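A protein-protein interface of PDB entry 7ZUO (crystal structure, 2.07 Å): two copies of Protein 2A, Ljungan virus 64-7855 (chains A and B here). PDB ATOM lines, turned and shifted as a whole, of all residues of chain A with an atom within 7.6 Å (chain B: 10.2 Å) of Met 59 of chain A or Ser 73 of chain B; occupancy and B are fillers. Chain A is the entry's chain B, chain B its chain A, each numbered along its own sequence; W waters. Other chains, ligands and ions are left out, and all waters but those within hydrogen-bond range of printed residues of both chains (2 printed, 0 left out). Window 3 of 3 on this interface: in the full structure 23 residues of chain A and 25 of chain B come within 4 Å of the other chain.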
ATOM      1  N   ASP A   5       0.758 -33.291  -6.216  1.00  0.00           N
ATOM      2  CA  ASP A   5       0.640 -31.846  -6.202  1.00  0.00           C
ATOM      3  C   ASP A   5       1.168 -31.296  -7.529  1.00  0.00           C
ATOM      4  O   ASP A   5       2.140 -31.816  -8.077  1.00  0.00           O
ATOM      5  CB  ASP A   5       1.389 -31.274  -5.001  1.00  0.00           C
ATOM      6  CG  ASP A   5       0.796 -31.665  -3.655  1.00  0.00           C
ATOM      7  OD1 ASP A   5      -0.412 -31.951  -3.604  1.00  0.00           O
ATOM      8  OD2 ASP A   5       1.567 -31.701  -2.672  1.00  0.00           O
ATOM      9  N   ILE A   6       0.559 -30.221  -8.037  1.00  0.00           N
ATOM     10  CA  ILE A   6       1.213 -29.448  -9.089  1.00  0.00           C
ATOM     11  C   ILE A   6       1.747 -28.135  -8.507  1.00  0.00           C
ATOM     12  O   ILE A   6       1.296 -27.675  -7.464  1.00  0.00           O
ATOM     13  CB  ILE A   6       0.261 -29.178 -10.268  1.00  0.00           C
ATOM     14  CG1 ILE A   6      -0.892 -28.265  -9.863  1.00  0.00           C
ATOM     15  CG2 ILE A   6      -0.234 -30.471 -10.873  1.00  0.00           C
ATOM     16  CD1 ILE A   6      -1.657 -27.738 -11.038  1.00  0.00           C
ATOM     17  N   GLU A   7       2.663 -27.510  -9.241  1.00  0.00           N
ATOM     18  CA  GLU A   7       3.248 -26.258  -8.827  1.00  0.00           C
ATOM     19  C   GLU A   7       2.792 -25.140  -9.774  1.00  0.00           C
ATOM     20  O   GLU A   7       3.131 -25.111 -10.973  1.00  0.00           O
ATOM     21  CB  GLU A   7       4.771 -26.355  -8.754  1.00  0.00           C
ATOM     22  CG  GLU A   7       5.342 -25.140  -8.034  1.00  0.00           C
ATOM     23  CD  GLU A   7       6.804 -24.843  -8.319  1.00  0.00           C
ATOM     24  OE1 GLU A   7       7.379 -25.582  -9.082  1.00  0.00           O
ATOM     25  OE2 GLU A   7       7.328 -23.813  -7.815  1.00  0.00           O
ATOM     26  N   LEU A   8       1.995 -24.241  -9.202  1.00  0.00           N
ATOM     27  CA  LEU A   8       1.638 -22.983  -9.841  1.00  0.00           C
ATOM     28  C   LEU A   8       2.813 -22.022  -9.697  1.00  0.00           C
ATOM     29  O   LEU A   8       3.376 -21.894  -8.607  1.00  0.00           O
ATOM     30  CB  LEU A   8       0.384 -22.480  -9.122  1.00  0.00           C
ATOM     31  CG  LEU A   8      -0.434 -21.387  -9.790  1.00  0.00           C
ATOM     32  CD1 LEU A   8      -0.962 -21.847 -11.144  1.00  0.00           C
ATOM     33  CD2 LEU A   8      -1.580 -20.951  -8.872  1.00  0.00           C
ATOM     34  N   VAL A   9       3.194 -21.376 -10.802  1.00  0.00           N
ATOM     35  CA  VAL A   9       4.292 -20.423 -10.814  1.00  0.00           C
ATOM     36  C   VAL A   9       3.846 -19.195 -11.610  1.00  0.00           C
ATOM     37  O   VAL A   9       2.822 -19.231 -12.286  1.00  0.00           O
ATOM     38  CB  VAL A   9       5.555 -21.059 -11.420  1.00  0.00           C
ATOM     39  CG1 VAL A   9       6.072 -22.245 -10.600  1.00  0.00           C
ATOM     40  CG2 VAL A   9       5.339 -21.474 -12.866  1.00  0.00           C
ATOM     41  N   TYR A  10       4.629 -18.117 -11.562  1.00  0.00           N
ATOM     42  CA  TYR A  10       4.310 -16.922 -12.330  1.00  0.00           C
ATOM     43  C   TYR A  10       5.566 -16.100 -12.632  1.00  0.00           C
ATOM     44  O   TYR A  10       6.595 -16.238 -11.965  1.00  0.00           O
ATOM     45  CB  TYR A  10       3.267 -16.050 -11.614  1.00  0.00           C
ATOM     46  CG  TYR A  10       3.746 -15.333 -10.377  1.00  0.00           C
ATOM     47  CD1 TYR A  10       4.475 -14.149 -10.444  1.00  0.00           C
ATOM     48  CD2 TYR A  10       3.479 -15.853  -9.125  1.00  0.00           C
ATOM     49  CE1 TYR A  10       4.946 -13.523  -9.297  1.00  0.00           C
ATOM     50  CE2 TYR A  10       3.922 -15.233  -7.967  1.00  0.00           C
ATOM     51  CZ  TYR A  10       4.664 -14.075  -8.057  1.00  0.00           C
ATOM     52  OH  TYR A  10       5.039 -13.486  -6.885  1.00  0.00           O
ATOM     53  N   TYR A  19       0.791 -16.603 -15.018  1.00  0.00           N
ATOM     54  CA  TYR A  19       0.847 -17.884 -14.344  1.00  0.00           C
ATOM     55  C   TYR A  19       1.150 -19.003 -15.330  1.00  0.00           C
ATOM     56  O   TYR A  19       0.804 -18.937 -16.523  1.00  0.00           O
ATOM     57  CB  TYR A  19      -0.458 -18.162 -13.597  1.00  0.00           C
ATOM     58  CG  TYR A  19      -0.586 -17.473 -12.267  1.00  0.00           C
ATOM     59  CD1 TYR A  19      -0.984 -16.155 -12.175  1.00  0.00           C
ATOM     60  CD2 TYR A  19      -0.255 -18.133 -11.091  1.00  0.00           C
ATOM     61  CE1 TYR A  19      -1.080 -15.520 -10.946  1.00  0.00           C
ATOM     62  CE2 TYR A  19      -0.353 -17.521  -9.850  1.00  0.00           C
ATOM     63  CZ  TYR A  19      -0.795 -16.215  -9.783  1.00  0.00           C
ATOM     64  OH  TYR A  19      -0.916 -15.572  -8.595  1.00  0.00           O
ATOM     65  N   GLY A  20       1.835 -20.012 -14.789  1.00  0.00           N
ATOM     66  CA  GLY A  20       2.124 -21.261 -15.474  1.00  0.00           C
ATOM     67  C   GLY A  20       2.049 -22.442 -14.497  1.00  0.00           C
ATOM     68  O   GLY A  20       1.908 -22.247 -13.285  1.00  0.00           O
ATOM     69  N   ILE A  21       2.121 -23.665 -15.047  1.00  0.00           N
ATOM     70  CA  ILE A  21       2.262 -24.875 -14.255  1.00  0.00           C
ATOM     71  C   ILE A  21       3.665 -25.429 -14.525  1.00  0.00           C
ATOM     72  O   ILE A  21       4.022 -25.739 -15.675  1.00  0.00           O
ATOM     73  CB  ILE A  21       1.181 -25.925 -14.580  1.00  0.00           C
ATOM     74  CG1 ILE A  21      -0.250 -25.384 -14.469  1.00  0.00           C
ATOM     75  CG2 ILE A  21       1.384 -27.184 -13.741  1.00  0.00           C
ATOM     76  CD1 ILE A  21      -0.572 -24.733 -13.155  1.00  0.00           C
ATOM     77  N   THR A  56       8.593 -17.447 -10.473  1.00  0.00           N
ATOM     78  CA  THR A  56       8.390 -17.390  -9.035  1.00  0.00           C
ATOM     79  C   THR A  56       7.371 -18.441  -8.603  1.00  0.00           C
ATOM     80  O   THR A  56       6.324 -18.631  -9.248  1.00  0.00           O
ATOM     81  CB  THR A  56       7.928 -16.000  -8.603  1.00  0.00           C
ATOM     82  OG1 THR A  56       8.943 -15.081  -8.993  1.00  0.00           O
ATOM     83  CG2 THR A  56       7.669 -15.896  -7.117  1.00  0.00           C
ATOM     84  N   HIS A  57       7.724 -19.154  -7.521  1.00  0.00           N
ATOM     85  CA  HIS A  57       6.829 -20.129  -6.922  1.00  0.00           C
ATOM     86  C   HIS A  57       5.575 -19.404  -6.418  1.00  0.00           C
ATOM     87  O   HIS A  57       5.666 -18.382  -5.737  1.00  0.00           O
ATOM     88  CB  HIS A  57       7.529 -20.894  -5.787  1.00  0.00           C
ATOM     89  CG  HIS A  57       6.591 -21.806  -5.067  1.00  0.00           C
ATOM     90  ND1 HIS A  57       6.125 -22.969  -5.611  1.00  0.00           N
ATOM     91  CD2 HIS A  57       5.947 -21.638  -3.869  1.00  0.00           C
ATOM     92  CE1 HIS A  57       5.248 -23.513  -4.758  1.00  0.00           C
ATOM     93  NE2 HIS A  57       5.135 -22.724  -3.672  1.00  0.00           N
ATOM     94  N   ALA A  58       4.386 -19.916  -6.767  1.00  0.00           N
ATOM     95  CA  ALA A  58       3.153 -19.300  -6.289  1.00  0.00           C
ATOM     96  C   ALA A  58       2.521 -20.193  -5.228  1.00  0.00           C
ATOM     97  O   ALA A  58       2.277 -19.770  -4.102  1.00  0.00           O
ATOM     98  CB  ALA A  58       2.199 -19.027  -7.437  1.00  0.00           C
ATOM     99  N   MET A  59       2.303 -21.455  -5.590  1.00  0.00           N
ATOM    100  CA  MET A  59       1.551 -22.343  -4.739  1.00  0.00           C
ATOM    101  C   MET A  59       1.719 -23.783  -5.187  1.00  0.00           C
ATOM    102  O   MET A  59       1.794 -24.062  -6.384  1.00  0.00           O
ATOM    103  CB  MET A  59       0.086 -21.946  -4.866  1.00  0.00           C
ATOM    104  CG  MET A  59      -0.799 -22.572  -3.888  1.00  0.00           C
ATOM    105  SD  MET A  59      -2.398 -21.774  -4.090  1.00  0.00           S
ATOM    106  CE  MET A  59      -3.255 -22.772  -2.875  1.00  0.00           C
ATOM    107  N   THR A  60       1.725 -24.687  -4.206  1.00  0.00           N
ATOM    108  CA  THR A  60       1.704 -26.111  -4.468  1.00  0.00           C
ATOM    109  C   THR A  60       0.387 -26.682  -3.952  1.00  0.00           C
ATOM    110  O   THR A  60       0.067 -26.549  -2.774  1.00  0.00           O
ATOM    111  CB  THR A  60       2.892 -26.805  -3.784  1.00  0.00           C
ATOM    112  OG1 THR A  60       4.079 -26.213  -4.304  1.00  0.00           O
ATOM    113  CG2 THR A  60       2.934 -28.309  -3.985  1.00  0.00           C
ATOM    114  N   ALA A  61      -0.346 -27.364  -4.831  1.00  0.00           N
ATOM    115  CA  ALA A  61      -1.588 -28.003  -4.438  1.00  0.00           C
ATOM    116  C   ALA A  61      -1.957 -29.033  -5.491  1.00  0.00           C
ATOM    117  O   ALA A  61      -1.480 -28.961  -6.629  1.00  0.00           O
ATOM    118  CB  ALA A  61      -2.674 -26.957  -4.275  1.00  0.00           C
ATOM    119  N   PRO A  62      -2.838 -30.006  -5.188  1.00  0.00           N
ATOM    120  CA  PRO A  62      -3.319 -30.900  -6.232  1.00  0.00           C
ATOM    121  C   PRO A  62      -4.089 -30.083  -7.275  1.00  0.00           C
ATOM    122  O   PRO A  62      -4.634 -29.004  -6.973  1.00  0.00           O
ATOM    123  CB  PRO A  62      -4.233 -31.881  -5.510  1.00  0.00           C
ATOM    124  CG  PRO A  62      -3.861 -31.721  -4.052  1.00  0.00           C
ATOM    125  CD  PRO A  62      -3.465 -30.269  -3.886  1.00  0.00           C
ATOM    126  N   TYR A  65      -7.598 -28.897  -6.521  1.00  0.00           N
ATOM    127  CA  TYR A  65      -7.778 -27.657  -5.784  1.00  0.00           C
ATOM    128  C   TYR A  65      -8.202 -26.545  -6.747  1.00  0.00           C
ATOM    129  O   TYR A  65      -9.033 -25.701  -6.414  1.00  0.00           O
ATOM    130  CB  TYR A  65      -6.490 -27.252  -5.049  1.00  0.00           C
ATOM    131  CG  TYR A  65      -6.565 -25.928  -4.330  1.00  0.00           C
ATOM    132  CD1 TYR A  65      -6.315 -24.742  -5.012  1.00  0.00           C
ATOM    133  CD2 TYR A  65      -6.900 -25.848  -2.989  1.00  0.00           C
ATOM    134  CE1 TYR A  65      -6.382 -23.515  -4.380  1.00  0.00           C
ATOM    135  CE2 TYR A  65      -6.984 -24.621  -2.341  1.00  0.00           C
ATOM    136  CZ  TYR A  65      -6.719 -23.452  -3.043  1.00  0.00           C
ATOM    137  OH  TYR A  65      -6.808 -22.204  -2.475  1.00  0.00           O
ATOM    138  N   PHE A  66      -7.580 -26.520  -7.927  1.00  0.00           N
ATOM    139  CA  PHE A  66      -7.760 -25.423  -8.861  1.00  0.00           C
ATOM    140  C   PHE A  66      -8.979 -25.672  -9.747  1.00  0.00           C
ATOM    141  O   PHE A  66      -9.795 -24.756  -9.930  1.00  0.00           O
ATOM    142  CB  PHE A  66      -6.462 -25.217  -9.653  1.00  0.00           C
ATOM    143  CG  PHE A  66      -5.249 -24.915  -8.808  1.00  0.00           C
ATOM    144  CD1 PHE A  66      -5.070 -23.658  -8.251  1.00  0.00           C
ATOM    145  CD2 PHE A  66      -4.318 -25.905  -8.524  1.00  0.00           C
ATOM    146  CE1 PHE A  66      -3.945 -23.382  -7.492  1.00  0.00           C
ATOM    147  CE2 PHE A  66      -3.175 -25.616  -7.793  1.00  0.00           C
ATOM    148  CZ  PHE A  66      -3.013 -24.369  -7.247  1.00  0.00           C
ATOM    149  N   LYS A  69     -12.412 -24.934  -8.466  1.00  0.00           N
ATOM    150  CA  LYS A  69     -12.717 -23.523  -8.284  1.00  0.00           C
ATOM    151  C   LYS A  69     -12.952 -22.797  -9.611  1.00  0.00           C
ATOM    152  O   LYS A  69     -13.889 -22.011  -9.712  1.00  0.00           O
ATOM    153  CB  LYS A  69     -11.589 -22.856  -7.495  1.00  0.00           C
ATOM    154  CG  LYS A  69     -11.488 -23.313  -6.044  1.00  0.00           C
ATOM    155  CD  LYS A  69     -10.261 -22.816  -5.319  1.00  0.00           C
ATOM    156  CE  LYS A  69     -10.190 -23.342  -3.905  1.00  0.00           C
ATOM    157  NZ  LYS A  69     -10.118 -24.824  -3.904  1.00  0.00           N
ATOM    158  N   TYR A  70     -12.060 -22.995 -10.587  1.00  0.00           N
ATOM    159  CA  TYR A  70     -11.938 -22.072 -11.718  1.00  0.00           C
ATOM    160  C   TYR A  70     -12.625 -22.603 -12.980  1.00  0.00           C
ATOM    161  O   TYR A  70     -12.804 -21.839 -13.931  1.00  0.00           O
ATOM    162  CB  TYR A  70     -10.474 -21.625 -11.890  1.00  0.00           C
ATOM    163  CG  TYR A  70     -10.050 -20.923 -10.632  1.00  0.00           C
ATOM    164  CD1 TYR A  70     -10.730 -19.803 -10.182  1.00  0.00           C
ATOM    165  CD2 TYR A  70      -9.082 -21.461  -9.805  1.00  0.00           C
ATOM    166  CE1 TYR A  70     -10.473 -19.243  -8.942  1.00  0.00           C
ATOM    167  CE2 TYR A  70      -8.783 -20.884  -8.579  1.00  0.00           C
ATOM    168  CZ  TYR A  70      -9.489 -19.787  -8.129  1.00  0.00           C
ATOM    169  OH  TYR A  70      -9.165 -19.251  -6.900  1.00  0.00           O
ATOM    170  N   THR B  67     -16.961 -17.658  -1.869  1.00  0.00           N
ATOM    171  CA  THR B  67     -15.796 -17.440  -1.021  1.00  0.00           C
ATOM    172  C   THR B  67     -14.723 -18.492  -1.283  1.00  0.00           C
ATOM    173  O   THR B  67     -13.531 -18.213  -1.225  1.00  0.00           O
ATOM    174  CB  THR B  67     -16.140 -17.420   0.470  1.00  0.00           C
ATOM    175  OG1 THR B  67     -16.694 -18.680   0.834  1.00  0.00           O
ATOM    176  CG2 THR B  67     -17.098 -16.303   0.794  1.00  0.00           C
ATOM    177  N   GLU B  68     -15.160 -19.708  -1.587  1.00  0.00           N
ATOM    178  CA  GLU B  68     -14.233 -20.778  -1.883  1.00  0.00           C
ATOM    179  C   GLU B  68     -13.310 -20.425  -3.060  1.00  0.00           C
ATOM    180  O   GLU B  68     -12.140 -20.832  -3.061  1.00  0.00           O
ATOM    181  CB  GLU B  68     -15.063 -22.029  -2.137  1.00  0.00           C
ATOM    182  CG  GLU B  68     -14.237 -23.228  -2.489  1.00  0.00           C
ATOM    183  CD  GLU B  68     -15.094 -24.479  -2.468  1.00  0.00           C
ATOM    184  OE1 GLU B  68     -15.650 -24.781  -1.359  1.00  0.00           O
ATOM    185  OE2 GLU B  68     -15.252 -25.102  -3.557  1.00  0.00           O
ATOM    186  N   LYS B  69     -13.835 -19.668  -4.047  1.00  0.00           N
ATOM    187  CA  LYS B  69     -13.108 -19.360  -5.273  1.00  0.00           C
ATOM    188  C   LYS B  69     -12.289 -18.075  -5.123  1.00  0.00           C
ATOM    189  O   LYS B  69     -11.228 -17.920  -5.751  1.00  0.00           O
ATOM    190  CB  LYS B  69     -14.088 -19.211  -6.445  1.00  0.00           C
ATOM    191  CG  LYS B  69     -14.944 -20.436  -6.740  1.00  0.00           C
ATOM    192  CD  LYS B  69     -16.093 -20.152  -7.692  1.00  0.00           C
ATOM    193  CE  LYS B  69     -16.799 -21.414  -8.155  1.00  0.00           C
ATOM    194  NZ  LYS B  69     -17.444 -22.128  -7.025  1.00  0.00           N
ATOM    195  N   TYR B  70     -12.753 -17.138  -4.283  1.00  0.00           N
ATOM    196  CA  TYR B  70     -12.202 -15.790  -4.332  1.00  0.00           C
ATOM    197  C   TYR B  70     -11.568 -15.331  -3.018  1.00  0.00           C
ATOM    198  O   TYR B  70     -10.982 -14.249  -2.987  1.00  0.00           O
ATOM    199  CB  TYR B  70     -13.286 -14.809  -4.803  1.00  0.00           C
ATOM    200  CG  TYR B  70     -13.854 -15.151  -6.163  1.00  0.00           C
ATOM    201  CD1 TYR B  70     -13.032 -15.551  -7.208  1.00  0.00           C
ATOM    202  CD2 TYR B  70     -15.218 -15.097  -6.405  1.00  0.00           C
ATOM    203  CE1 TYR B  70     -13.557 -15.900  -8.446  1.00  0.00           C
ATOM    204  CE2 TYR B  70     -15.757 -15.410  -7.651  1.00  0.00           C
ATOM    205  CZ  TYR B  70     -14.926 -15.811  -8.673  1.00  0.00           C
ATOM    206  OH  TYR B  70     -15.444 -16.128  -9.919  1.00  0.00           O
ATOM    207  N   VAL B  71     -11.758 -16.102  -1.947  1.00  0.00           N
ATOM    208  CA  VAL B  71     -11.216 -15.795  -0.630  1.00  0.00           C
ATOM    209  C   VAL B  71     -10.408 -17.020  -0.236  1.00  0.00           C
ATOM    210  O   VAL B  71     -10.900 -17.899   0.470  1.00  0.00           O
ATOM    211  CB  VAL B  71     -12.317 -15.494   0.420  1.00  0.00           C
ATOM    212  CG1 VAL B  71     -11.725 -15.035   1.750  1.00  0.00           C
ATOM    213  CG2 VAL B  71     -13.324 -14.469  -0.064  1.00  0.00           C
ATOM    214  N   ASN B  72      -9.191 -17.125  -0.764  1.00  0.00           N
ATOM    215  CA  ASN B  72      -8.464 -18.373  -0.610  1.00  0.00           C
ATOM    216  C   ASN B  72      -6.984 -18.084  -0.753  1.00  0.00           C
ATOM    217  O   ASN B  72      -6.599 -16.942  -0.954  1.00  0.00           O
ATOM    218  CB  ASN B  72      -8.986 -19.459  -1.561  1.00  0.00           C
ATOM    219  CG  ASN B  72      -8.647 -19.240  -3.022  1.00  0.00           C
ATOM    220  OD1 ASN B  72      -7.603 -18.678  -3.319  1.00  0.00           O
ATOM    221  ND2 ASN B  72      -9.469 -19.747  -3.937  1.00  0.00           N
ATOM    222  N   SER B  73      -6.186 -19.147  -0.652  1.00  0.00           N
ATOM    223  CA  SER B  73      -4.736 -19.028  -0.568  1.00  0.00           C
ATOM    224  C   SER B  73      -4.126 -18.658  -1.922  1.00  0.00           C
ATOM    225  O   SER B  73      -3.058 -18.055  -1.963  1.00  0.00           O
ATOM    226  CB  SER B  73      -4.131 -20.276   0.039  1.00  0.00           C
ATOM    227  OG  SER B  73      -4.580 -20.462   1.389  1.00  0.00           O
ATOM    228  N   MET B  74      -4.796 -18.972  -3.030  1.00  0.00           N
ATOM    229  CA  MET B  74      -4.213 -18.681  -4.322  1.00  0.00           C
ATOM    230  C   MET B  74      -4.423 -17.203  -4.650  1.00  0.00           C
ATOM    231  O   MET B  74      -3.553 -16.584  -5.254  1.00  0.00           O
ATOM    232  CB  MET B  74      -4.845 -19.532  -5.438  1.00  0.00           C
ATOM    233  CG  MET B  74      -4.185 -19.320  -6.792  1.00  0.00           C
ATOM    234  SD  MET B  74      -5.143 -19.945  -8.198  1.00  0.00           S
ATOM    235  CE  MET B  74      -6.248 -18.563  -8.479  1.00  0.00           C
ATOM    236  N   VAL B  75      -5.588 -16.666  -4.282  1.00  0.00           N
ATOM    237  CA  VAL B  75      -6.009 -15.332  -4.699  1.00  0.00           C
ATOM    238  C   VAL B  75      -5.405 -14.262  -3.792  1.00  0.00           C
ATOM    239  O   VAL B  75      -6.045 -13.773  -2.873  1.00  0.00           O
ATOM    240  CB  VAL B  75      -7.544 -15.252  -4.774  1.00  0.00           C
ATOM    241  CG1 VAL B  75      -8.035 -13.858  -5.094  1.00  0.00           C
ATOM    242  CG2 VAL B  75      -8.061 -16.251  -5.804  1.00  0.00           C
ATOM    243  N   GLY B  76      -4.177 -13.850  -4.093  1.00  0.00           N
ATOM    244  CA  GLY B  76      -3.557 -12.755  -3.361  1.00  0.00           C
ATOM    245  C   GLY B  76      -4.269 -11.427  -3.618  1.00  0.00           C
ATOM    246  O   GLY B  76      -4.853 -11.221  -4.678  1.00  0.00           O
ATOM    247  N   SER B  77      -4.192 -10.503  -2.659  1.00  0.00           N
ATOM    248  CA  SER B  77      -4.860  -9.218  -2.797  1.00  0.00           C
ATOM    249  C   SER B  77      -4.166  -8.219  -1.895  1.00  0.00           C
ATOM    250  O   SER B  77      -3.926  -8.546  -0.749  1.00  0.00           O
ATOM    251  CB  SER B  77      -6.333  -9.322  -2.422  1.00  0.00           C
ATOM    252  OG  SER B  77      -6.961  -8.054  -2.366  1.00  0.00           O
ATOM    253  N   LEU B 112     -13.779  -8.920  -2.127  1.00  0.00           N
ATOM    254  CA  LEU B 112     -12.989  -9.816  -2.957  1.00  0.00           C
ATOM    255  C   LEU B 112     -13.903 -10.541  -3.948  1.00  0.00           C
ATOM    256  O   LEU B 112     -13.510 -10.847  -5.065  1.00  0.00           O
ATOM    257  CB  LEU B 112     -12.248 -10.827  -2.081  1.00  0.00           C
ATOM    258  CG  LEU B 112     -10.973 -10.323  -1.403  1.00  0.00           C
ATOM    259  CD1 LEU B 112     -10.435 -11.353  -0.423  1.00  0.00           C
ATOM    260  CD2 LEU B 112      -9.923  -9.997  -2.433  1.00  0.00           C
HETATM  261  O   HOH W   1      -1.255 -17.284  -6.547  1.00  0.00           O
HETATM  262  O   HOH W   2     -12.477 -26.133  -4.070  1.00  0.00           O
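ND2 of Asn 72 of chain B is in hydrogen-bond range of OH of Tyr 70 of chain A.
The backbone carbonyl oxygen of Lys 69 of chain B lies within hydrogen-bond range of the side-chain hydroxyl of Tyr 70 of chain A (2.7 Å).
The backbone carbonyl oxygen (O) of Lys 69 of chain B sits at hydrogen-bond distance from the side-chain amide nitrogen (ND2) of Asn 72 of chain B (3.1 Å).
The backbone NH (N) of Val 75 of chain B sits at hydrogen-bond distance from the side-chain amide oxygen (OD1) of Asn 72 of chain B.
OD1 of Asn 72 of chain B sits at hydrogen-bond distance from N of Met 74 of chain B.
The side-chain amino group (NZ) of Lys 69 of chain A sits at hydrogen-bond distance from the backbone carbonyl oxygen (O) of Tyr 65 of chain A, at 2.9 Å.
The backbone carbonyl oxygen (O) of Met 59 of chain A is in hydrogen-bond range of the backbone NH (N) of Leu 8 of chain A (2.8 Å).
The backbone carbonyl oxygen (O) of Glu 68 of chain B sits at hydrogen-bond distance from the side-chain amide nitrogen (ND2) of Asn 72 of chain B, at 3.0 Å.
Among the printed residues, pairs that only touch across the chains: Leu 8 of chain A with Met 74 of chain B (3.7 Å), Met 59 of chain A with Ser 73 of chain B (3.9 Å), Met 59 of chain A with Met 74 of chain B (3.6 Å), Tyr 65 of chain A with Asn 72 of chain B (3.5 Å), Tyr 65 of chain A with Ser 73 of chain B (3.6 Å), Tyr 65 of chain A with Met 74 of chain B (3.8 Å), Phe 66 of chain A with Met 74 of chain B (3.7 Å), Lys 69 of chain A with Glu 68 of chain B (3.3 Å), Lys 69 of chain A with Lys 69 of chain B (3.4 Å), Lys 69 of chain A with Asn 72 of chain B (3.5 Å), Tyr 70 of chain A with Met 74 of chain B (3.4 Å) and Tyr 70 of chain A with Val 75 of chain B (3.4 Å).
Of the printed residues of chain B, Met 59 of chain A touches Ser 73 (3.9 Å) and Met 74 (3.6 Å).
Printed residues of chain A within 4 Å of Met 74 of chain B: Leu 8, Met 59, Tyr 65, Phe 66 and Tyr 70.
Of the printed residues of chain B, Tyr 65 of chain A touches Asn 72 (3.5 Å), Ser 73 (3.6 Å) and Met 74 (3.8 Å).
Printed residues of chain B within 4 Å of Phe 66 of chain A: Met 74.
Of the printed residues of chain B, Tyr 70 of chain A touches Lys 69 (2.7 Å), Asn 72 (3.0 Å), Met 74 (3.4 Å) and Val 75 (3.4 Å).
Of the printed residues of chain B, Lys 69 of chain A touches Glu 68 (3.3 Å), Lys 69 (3.4 Å) and Asn 72 (3.5 Å).
The nearest printed residue of chain A that does not touch Asn 72 of chain B is Met 59 of chain A (6.0 Å).
Hydrophobic or aromatic side chains of chain B that line the printed part of chain A: Met 74 and Val 75.
Of the 20 printed residues of chain A, 6 touch a printed residue of chain B.
Among the printed residues, 14 pairs touch across the chains.
Lys 69 of chain B touches its own counterpart, Lys 69 of chain A.
Tyr 70 of chain A touches Lys 69 of chain B, but with the chains exchanged Lys 69 of chain A does not touch Tyr 70 of chain B (6.1 Å).
Of the 14 pairs that touch across the chains among the printed residues, 1 has its exchanged pair printed and touching as well.
Water W1 bridges OH of Tyr 19 of chain A (2.7 Å) and O of Met 74 of chain B (2.7 Å).
Water W2 lies within hydrogen-bond range of NZ of Lys 69 of chain A (2.7 Å) and OE2 of Glu 68 of chain B (3.0 Å).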
